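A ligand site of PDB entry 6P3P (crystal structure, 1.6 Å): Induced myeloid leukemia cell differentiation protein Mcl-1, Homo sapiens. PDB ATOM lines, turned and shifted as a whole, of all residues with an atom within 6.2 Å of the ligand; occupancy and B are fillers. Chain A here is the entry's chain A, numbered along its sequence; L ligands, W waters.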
ATOM      1  N   VAL A  46      19.441  22.474   4.674  1.00  0.00           N
ATOM      2  CA  VAL A  46      18.724  23.632   4.167  1.00  0.00           C
ATOM      3  C   VAL A  46      17.222  23.326   4.079  1.00  0.00           C
ATOM      4  O   VAL A  46      16.391  24.169   4.422  1.00  0.00           O
ATOM      5  CB  VAL A  46      19.279  24.087   2.798  1.00  0.00           C
ATOM      6  CG1 VAL A  46      18.572  25.333   2.316  1.00  0.00           C
ATOM      7  CG2 VAL A  46      20.777  24.359   2.907  1.00  0.00           C
ATOM      8  N   VAL A  50      13.849  25.080   5.604  1.00  0.00           N
ATOM      9  CA  VAL A  50      12.763  25.561   4.763  1.00  0.00           C
ATOM     10  C   VAL A  50      11.431  25.002   5.254  1.00  0.00           C
ATOM     11  O   VAL A  50      10.463  25.745   5.372  1.00  0.00           O
ATOM     12  CB  VAL A  50      13.013  25.230   3.263  1.00  0.00           C
ATOM     13  CG1 VAL A  50      11.764  25.462   2.423  1.00  0.00           C
ATOM     14  CG2 VAL A  50      14.156  26.083   2.732  1.00  0.00           C
ATOM     15  N   HIS A  54       8.450  27.352   6.415  1.00  0.00           N
ATOM     16  CA  HIS A  54       7.377  27.384   5.394  1.00  0.00           C
ATOM     17  C   HIS A  54       6.148  26.539   5.717  1.00  0.00           C
ATOM     18  O   HIS A  54       5.271  26.360   4.862  1.00  0.00           O
ATOM     19  CB  HIS A  54       7.918  26.890   4.055  1.00  0.00           C
ATOM     20  CG  HIS A  54       8.875  27.830   3.424  1.00  0.00           C
ATOM     21  ND1 HIS A  54       9.945  28.369   4.094  1.00  0.00           N
ATOM     22  CD2 HIS A  54       8.907  28.348   2.173  1.00  0.00           C
ATOM     23  CE1 HIS A  54      10.605  29.186   3.287  1.00  0.00           C
ATOM     24  NE2 HIS A  54       9.990  29.181   2.116  1.00  0.00           N
ATOM     25  N   ALA A  57       2.652  27.994   4.675  1.00  0.00           N
ATOM     26  CA  ALA A  57       2.478  28.034   3.237  1.00  0.00           C
ATOM     27  C   ALA A  57       2.313  26.626   2.659  1.00  0.00           C
ATOM     28  O   ALA A  57       1.466  26.416   1.801  1.00  0.00           O
ATOM     29  CB  ALA A  57       3.652  28.747   2.565  1.00  0.00           C
ATOM     30  N   PHE A  58       3.116  25.690   3.168  1.00  0.00           N
ATOM     31  CA  PHE A  58       3.047  24.304   2.710  1.00  0.00           C
ATOM     32  C   PHE A  58       1.724  23.635   3.085  1.00  0.00           C
ATOM     33  O   PHE A  58       1.118  22.944   2.249  1.00  0.00           O
ATOM     34  CB  PHE A  58       4.248  23.480   3.238  1.00  0.00           C
ATOM     35  CG  PHE A  58       5.581  23.804   2.590  1.00  0.00           C
ATOM     36  CD1 PHE A  58       5.736  24.754   1.561  1.00  0.00           C
ATOM     37  CD2 PHE A  58       6.693  23.081   2.980  1.00  0.00           C
ATOM     38  CE1 PHE A  58       6.992  24.982   0.982  1.00  0.00           C
ATOM     39  CE2 PHE A  58       7.929  23.295   2.399  1.00  0.00           C
ATOM     40  CZ  PHE A  58       8.085  24.246   1.400  1.00  0.00           C
ATOM     41  N   MET A  61      -0.937  25.032   0.716  1.00  0.00           N
ATOM     42  CA  MET A  61      -0.863  24.427  -0.597  1.00  0.00           C
ATOM     43  C   MET A  61      -1.373  22.990  -0.564  1.00  0.00           C
ATOM     44  O   MET A  61      -2.140  22.604  -1.444  1.00  0.00           O
ATOM     45  CB  MET A  61       0.582  24.487  -1.118  1.00  0.00           C
ATOM     46  CG  MET A  61       0.756  24.035  -2.554  1.00  0.00           C
ATOM     47  SD  MET A  61      -0.078  25.064  -3.770  1.00  0.00           S
ATOM     48  CE  MET A  61       0.957  26.522  -3.740  1.00  0.00           C
ATOM     49  N   MET A  80       2.404  21.927 -10.306  1.00  0.00           N
ATOM     50  CA  MET A  80       3.669  22.420  -9.787  1.00  0.00           C
ATOM     51  C   MET A  80       4.527  23.111 -10.836  1.00  0.00           C
ATOM     52  O   MET A  80       5.304  23.978 -10.483  1.00  0.00           O
ATOM     53  CB  MET A  80       4.454  21.329  -9.041  1.00  0.00           C
ATOM     54  CG  MET A  80       3.742  20.818  -7.785  1.00  0.00           C
ATOM     55  SD  MET A  80       3.179  22.066  -6.609  1.00  0.00           S
ATOM     56  CE  MET A  80       4.749  22.791  -6.133  1.00  0.00           C
ATOM     57  N   VAL A  83       3.057  26.554 -10.404  1.00  0.00           N
ATOM     58  CA  VAL A  83       3.473  27.137  -9.126  1.00  0.00           C
ATOM     59  C   VAL A  83       4.969  27.476  -9.143  1.00  0.00           C
ATOM     60  O   VAL A  83       5.374  28.597  -8.842  1.00  0.00           O
ATOM     61  CB  VAL A  83       3.151  26.212  -7.923  1.00  0.00           C
ATOM     62  CG1 VAL A  83       3.740  26.749  -6.629  1.00  0.00           C
ATOM     63  CG2 VAL A  83       1.637  26.023  -7.768  1.00  0.00           C
ATOM     64  N   PHE A  84       5.793  26.496  -9.508  1.00  0.00           N
ATOM     65  CA  PHE A  84       7.243  26.668  -9.503  1.00  0.00           C
ATOM     66  C   PHE A  84       7.719  27.728 -10.503  1.00  0.00           C
ATOM     67  O   PHE A  84       8.599  28.529 -10.171  1.00  0.00           O
ATOM     68  CB  PHE A  84       7.935  25.338  -9.772  1.00  0.00           C
ATOM     69  CG  PHE A  84       9.426  25.416  -9.767  1.00  0.00           C
ATOM     70  CD1 PHE A  84      10.109  25.823  -8.629  1.00  0.00           C
ATOM     71  CD2 PHE A  84      10.143  25.084 -10.893  1.00  0.00           C
ATOM     72  CE1 PHE A  84      11.488  25.894  -8.620  1.00  0.00           C
ATOM     73  CE2 PHE A  84      11.521  25.150 -10.898  1.00  0.00           C
ATOM     74  CZ  PHE A  84      12.196  25.569  -9.756  1.00  0.00           C
ATOM     75  N   SER A  85       7.129  27.762 -11.690  1.00  0.00           N
ATOM     76  CA  SER A  85       7.510  28.749 -12.721  1.00  0.00           C
ATOM     77  C   SER A  85       7.054  30.175 -12.417  1.00  0.00           C
ATOM     78  O   SER A  85       7.573  31.119 -13.014  1.00  0.00           O
ATOM     79  CB  SER A  85       6.982  28.335 -14.095  1.00  0.00           C
ATOM     80  OG  SER A  85       7.495  27.079 -14.498  1.00  0.00           O
ATOM     81  N   ASP A  86       6.107  30.336 -11.488  1.00  0.00           N
ATOM     82  CA  ASP A  86       5.518  31.638 -11.148  1.00  0.00           C
ATOM     83  C   ASP A  86       6.362  32.386 -10.102  1.00  0.00           C
ATOM     84  O   ASP A  86       5.880  32.786  -9.037  1.00  0.00           O
ATOM     85  CB  ASP A  86       4.082  31.413 -10.637  1.00  0.00           C
ATOM     86  CG  ASP A  86       3.243  32.672 -10.627  1.00  0.00           C
ATOM     87  OD1 ASP A  86       3.486  33.576 -11.464  1.00  0.00           O
ATOM     88  OD2 ASP A  86       2.312  32.740  -9.798  1.00  0.00           O
ATOM     89  N   ASN A  90      15.909  30.679  -8.523  1.00  0.00           N
ATOM     90  CA  ASN A  90      17.174  30.695  -7.821  1.00  0.00           C
ATOM     91  C   ASN A  90      17.241  29.419  -7.030  1.00  0.00           C
ATOM     92  O   ASN A  90      16.273  28.655  -7.010  1.00  0.00           O
ATOM     93  CB  ASN A  90      17.308  31.950  -6.945  1.00  0.00           C
ATOM     94  CG  ASN A  90      16.092  32.199  -6.071  1.00  0.00           C
ATOM     95  OD1 ASN A  90      15.572  31.300  -5.416  1.00  0.00           O
ATOM     96  ND2 ASN A  90      15.650  33.464  -6.038  1.00  0.00           N
ATOM     97  N   TRP A  91      18.384  29.152  -6.419  1.00  0.00           N
ATOM     98  CA  TRP A  91      18.576  27.915  -5.661  1.00  0.00           C
ATOM     99  C   TRP A  91      17.611  27.811  -4.473  1.00  0.00           C
ATOM    100  O   TRP A  91      17.184  26.719  -4.130  1.00  0.00           O
ATOM    101  CB  TRP A  91      20.026  27.768  -5.185  1.00  0.00           C
ATOM    102  CG  TRP A  91      20.986  27.333  -6.234  1.00  0.00           C
ATOM    103  CD1 TRP A  91      22.100  28.009  -6.663  1.00  0.00           C
ATOM    104  CD2 TRP A  91      20.960  26.112  -6.964  1.00  0.00           C
ATOM    105  NE1 TRP A  91      22.761  27.280  -7.613  1.00  0.00           N
ATOM    106  CE2 TRP A  91      22.085  26.111  -7.823  1.00  0.00           C
ATOM    107  CE3 TRP A  91      20.088  25.009  -7.000  1.00  0.00           C
ATOM    108  CZ2 TRP A  91      22.364  25.061  -8.694  1.00  0.00           C
ATOM    109  CZ3 TRP A  91      20.367  23.959  -7.871  1.00  0.00           C
ATOM    110  CH2 TRP A  91      21.505  23.993  -8.698  1.00  0.00           C
ATOM    111  N   GLY A  92      17.282  28.953  -3.874  1.00  0.00           N
ATOM    112  CA  GLY A  92      16.283  28.982  -2.808  1.00  0.00           C
ATOM    113  C   GLY A  92      14.924  28.459  -3.222  1.00  0.00           C
ATOM    114  O   GLY A  92      14.323  27.649  -2.518  1.00  0.00           O
ATOM    115  N   ARG A  93      14.431  28.914  -4.372  1.00  0.00           N
ATOM    116  CA  ARG A  93      13.138  28.419  -4.890  1.00  0.00           C
ATOM    117  C   ARG A  93      13.207  26.910  -5.224  1.00  0.00           C
ATOM    118  O   ARG A  93      12.252  26.165  -5.022  1.00  0.00           O
ATOM    119  CB  ARG A  93      12.701  29.203  -6.119  1.00  0.00           C
ATOM    120  CG  ARG A  93      11.234  29.000  -6.439  1.00  0.00           C
ATOM    121  CD  ARG A  93      10.767  29.836  -7.613  1.00  0.00           C
ATOM    122  NE  ARG A  93       9.314  29.740  -7.778  1.00  0.00           N
ATOM    123  CZ  ARG A  93       8.412  30.434  -7.092  1.00  0.00           C
ATOM    124  NH1 ARG A  93       8.763  31.314  -6.138  1.00  0.00           N
ATOM    125  NH2 ARG A  93       7.116  30.258  -7.349  1.00  0.00           N
ATOM    126  N   ILE A  94      14.349  26.476  -5.735  1.00  0.00           N
ATOM    127  CA  ILE A  94      14.562  25.054  -6.068  1.00  0.00           C
ATOM    128  C   ILE A  94      14.530  24.198  -4.797  1.00  0.00           C
ATOM    129  O   ILE A  94      13.878  23.142  -4.755  1.00  0.00           O
ATOM    130  CB  ILE A  94      15.869  24.866  -6.885  1.00  0.00           C
ATOM    131  CG1 ILE A  94      15.664  25.459  -8.284  1.00  0.00           C
ATOM    132  CG2 ILE A  94      16.271  23.400  -6.981  1.00  0.00           C
ATOM    133  CD1 ILE A  94      16.935  25.682  -9.066  1.00  0.00           C
ATOM    134  N   VAL A  95      15.186  24.660  -3.732  1.00  0.00           N
ATOM    135  CA  VAL A  95      15.108  23.980  -2.447  1.00  0.00           C
ATOM    136  C   VAL A  95      13.661  23.963  -1.927  1.00  0.00           C
ATOM    137  O   VAL A  95      13.229  22.966  -1.372  1.00  0.00           O
ATOM    138  CB  VAL A  95      16.047  24.580  -1.358  1.00  0.00           C
ATOM    139  CG1 VAL A  95      15.773  23.929   0.010  1.00  0.00           C
ATOM    140  CG2 VAL A  95      17.485  24.355  -1.750  1.00  0.00           C
ATOM    141  N   THR A  96      12.937  25.065  -2.116  1.00  0.00           N
ATOM    142  CA  THR A  96      11.553  25.134  -1.662  1.00  0.00           C
ATOM    143  C   THR A  96      10.712  24.059  -2.364  1.00  0.00           C
ATOM    144  O   THR A  96       9.925  23.361  -1.725  1.00  0.00           O
ATOM    145  CB  THR A  96      10.988  26.555  -1.865  1.00  0.00           C
ATOM    146  OG1 THR A  96      11.811  27.470  -1.129  1.00  0.00           O
ATOM    147  CG2 THR A  96       9.540  26.639  -1.363  1.00  0.00           C
ATOM    148  N   LEU A  97      10.915  23.921  -3.667  1.00  0.00           N
ATOM    149  CA  LEU A  97      10.205  22.878  -4.422  1.00  0.00           C
ATOM    150  C   LEU A  97      10.462  21.488  -3.870  1.00  0.00           C
ATOM    151  O   LEU A  97       9.544  20.695  -3.686  1.00  0.00           O
ATOM    152  CB  LEU A  97      10.596  22.931  -5.903  1.00  0.00           C
ATOM    153  CG  LEU A  97      10.013  21.815  -6.782  1.00  0.00           C
ATOM    154  CD1 LEU A  97       8.518  21.983  -6.900  1.00  0.00           C
ATOM    155  CD2 LEU A  97      10.667  21.803  -8.149  1.00  0.00           C
ATOM    156  N   ILE A  98      11.730  21.169  -3.628  1.00  0.00           N
ATOM    157  CA  ILE A  98      12.115  19.843  -3.156  1.00  0.00           C
ATOM    158  C   ILE A  98      11.633  19.626  -1.716  1.00  0.00           C
ATOM    159  O   ILE A  98      11.164  18.537  -1.359  1.00  0.00           O
ATOM    160  CB  ILE A  98      13.632  19.637  -3.298  1.00  0.00           C
ATOM    161  CG1 ILE A  98      14.018  19.640  -4.796  1.00  0.00           C
ATOM    162  CG2 ILE A  98      14.099  18.344  -2.650  1.00  0.00           C
ATOM    163  CD1 ILE A  98      15.504  19.787  -5.025  1.00  0.00           C
ATOM    164  N   PHE A 100       9.021  21.117  -0.368  1.00  0.00           N
ATOM    165  CA  PHE A 100       7.586  20.866  -0.464  1.00  0.00           C
ATOM    166  C   PHE A 100       7.342  19.394  -0.810  1.00  0.00           C
ATOM    167  O   PHE A 100       6.479  18.752  -0.207  1.00  0.00           O
ATOM    168  CB  PHE A 100       6.894  21.805  -1.448  1.00  0.00           C
ATOM    169  CG  PHE A 100       5.408  21.587  -1.533  1.00  0.00           C
ATOM    170  CD1 PHE A 100       4.599  21.804  -0.407  1.00  0.00           C
ATOM    171  CD2 PHE A 100       4.804  21.144  -2.696  1.00  0.00           C
ATOM    172  CE1 PHE A 100       3.235  21.588  -0.456  1.00  0.00           C
ATOM    173  CE2 PHE A 100       3.433  20.934  -2.756  1.00  0.00           C
ATOM    174  CZ  PHE A 100       2.645  21.150  -1.637  1.00  0.00           C
ATOM    175  N   PHE A 149      25.412  26.557  -1.249  1.00  0.00           N
ATOM    176  CA  PHE A 149      24.992  26.456   0.144  1.00  0.00           C
ATOM    177  C   PHE A 149      26.110  26.123   1.132  1.00  0.00           C
ATOM    178  O   PHE A 149      25.862  26.008   2.324  1.00  0.00           O
ATOM    179  CB  PHE A 149      23.829  25.463   0.274  1.00  0.00           C
ATOM    180  CG  PHE A 149      22.538  25.970  -0.302  1.00  0.00           C
ATOM    181  CD1 PHE A 149      21.886  27.055   0.293  1.00  0.00           C
ATOM    182  CD2 PHE A 149      21.965  25.391  -1.434  1.00  0.00           C
ATOM    183  CE1 PHE A 149      20.691  27.540  -0.221  1.00  0.00           C
ATOM    184  CE2 PHE A 149      20.769  25.885  -1.952  1.00  0.00           C
ATOM    185  CZ  PHE A 149      20.140  26.955  -1.344  1.00  0.00           C
HETATM  186  C1  LIG L   1      15.098  32.619  -2.427  1.00  0.00           C
HETATM  187  C2  LIG L   1      13.564  31.641  -0.730  1.00  0.00           C
HETATM  188  C3  LIG L   1      12.962  30.367  -0.244  1.00  0.00           C
HETATM  189  C4  LIG L   1      14.852  29.866   1.266  1.00  0.00           C
HETATM  190  C5  LIG L   1      15.427  28.704   0.764  1.00  0.00           C
HETATM  191  C6  LIG L   1      16.793  28.475   0.915  1.00  0.00           C
HETATM  192  C7  LIG L   1      17.605  29.403   1.577  1.00  0.00           C
HETATM  193  C8  LIG L   1      17.024  30.567   2.086  1.00  0.00           C
HETATM  194  C9  LIG L   1      15.664  30.803   1.925  1.00  0.00           C
HETATM  195  C10 LIG L   1      10.842  30.480  -1.467  1.00  0.00           C
HETATM  196  C11 LIG L   1       7.100  30.289  -0.774  1.00  0.00           C
HETATM  197  C12 LIG L   1       6.968  30.391  -2.146  1.00  0.00           C
HETATM  198  C13 LIG L   1       5.177  27.649  -2.795  1.00  0.00           C
HETATM  199  C14 LIG L   1       6.134  27.518  -3.813  1.00  0.00           C
HETATM  200  C15 LIG L   1       6.657  26.263  -4.133  1.00  0.00           C
HETATM  201  C16 LIG L   1       6.209  25.139  -3.434  1.00  0.00           C
HETATM  202  C17 LIG L   1       5.266  25.280  -2.421  1.00  0.00           C
HETATM  203  F1  LIG L   1       8.858  25.964  -4.717  1.00  0.00           F
HETATM  204  C18 LIG L   1       7.655  26.118  -5.221  1.00  0.00           C
HETATM  205  F2  LIG L   1       7.671  27.163  -6.012  1.00  0.00           F
HETATM  206  F3  LIG L   1       7.358  25.063  -5.946  1.00  0.00           F
HETATM  207  C19 LIG L   1       4.757  26.545  -2.105  1.00  0.00           C
HETATM  208 CL1  LIG L   1       3.609  26.682  -0.874  1.00  0.00          CL
HETATM  209  N1  LIG L   1       4.661  28.957  -2.398  1.00  0.00           N
HETATM  210  S1  LIG L   1       5.480  30.410  -2.881  1.00  0.00           S
HETATM  211  O1  LIG L   1       5.665  30.522  -4.284  1.00  0.00           O
HETATM  212  O2  LIG L   1       4.721  31.490  -2.306  1.00  0.00           O
HETATM  213  C20 LIG L   1       6.084  30.177   0.349  1.00  0.00           C
HETATM  214  C21 LIG L   1       8.433  30.305  -0.355  1.00  0.00           C
HETATM  215  S2  LIG L   1       8.489  30.490  -2.851  1.00  0.00           S
HETATM  216  C22 LIG L   1       9.337  30.437  -1.408  1.00  0.00           C
HETATM  217  O3  LIG L   1      11.417  30.546  -2.543  1.00  0.00           O
HETATM  218  N2  LIG L   1      11.511  30.413  -0.321  1.00  0.00           N
HETATM  219  O4  LIG L   1      13.114  32.737  -0.416  1.00  0.00           O
HETATM  220  O5  LIG L   1      14.688  31.532  -1.614  1.00  0.00           O
HETATM  221  C23 LIG L   1      13.380  30.109   1.118  1.00  0.00           C
HETATM  222  O   HOH W   1      13.068  35.318  -1.242  1.00  0.00           O
HETATM  223  O   HOH W   2      10.873  32.251  -4.444  1.00  0.00           O
HETATM  224  O   HOH W   3       2.459  29.845  -1.066  1.00  0.00           O
HETATM  225  O   HOH W   4      14.722  35.344  -3.914  1.00  0.00           O
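NE2 of His 54 lies within hydrogen-bond range of N2 of the ligand, 3.1 Å away. S2 of the ligand lies close to NH1 of Arg 93, at 3.4 Å. The side-chain hydroxyl (OG1) of Thr 96 sits at hydrogen-bond distance from a nitrogen (N2) of the ligand (3.1 Å).
The side-chain amide oxygen (OD1) of Asn 90 sits at hydrogen-bond distance from the backbone NH (N) of Arg 93. The guanidinium group (NE) of Arg 93 lies within hydrogen-bond range of the backbone carbonyl oxygen (O) of Phe 84, at 2.8 Å. The guanidinium group (NH2) of Arg 93 is in hydrogen-bond range of the backbone carbonyl oxygen (O) of Asp 86, 3.3 Å away. The side-chain amide oxygen (OD1) of Asn 90 lies close to the backbone NH (N) of Gly 92, at 3.3 Å. The backbone carbonyl oxygen (O) of Val 50 is in hydrogen-bond range of a ring nitrogen (ND1) of His 54 (3.0 Å). The backbone carbonyl oxygen (O) of Gly 92 lies within hydrogen-bond range of the side-chain hydroxyl (OG1) of Thr 96, at 2.9 Å. The guanidinium group of Arg 93 sits at hydrogen-bond distance from the backbone carbonyl oxygen of Val 83.
The backbone NH of Leu 97 sits close to a fluorine (F1) of the ligand (3.1 Å). Val 46 touches the ligand (CG1 to C6, 3.9 Å). CG2 of Val 50 touches C5 of the ligand, at 3.5 Å. Ala 57 touches the ligand (O to CL1, 3.4 Å). Phe 58 touches the ligand (CD1 to CL1, 3.8 Å). Met 61 touches the ligand. Met 80 touches the ligand. Val 83 touches the ligand. Phe 84 touches the ligand. Asn 90 touches the ligand. Gly 92 touches the ligand (CA to O5, 3.2 Å). CG of Phe 100 touches C17 of the ligand (3.8 Å). Hydrophobic or aromatic side chains within 4 Å of the ligand: Val 46, Val 50, His 54, Ala 57, Phe 58, Met 61, Met 80, Val 83, Phe 84, Leu 97 and Phe 100. Within 4 Å of the ligand: Val 46, Val 50, His 54, Ala 57, Phe 58, Met 61, Met 80, Val 83, Phe 84, Asn 90, Gly 92, Arg 93, Thr 96, Leu 97 and Phe 100.
Water W2 lies within hydrogen-bond range of O3 of the ligand and NH1 of Arg 93.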
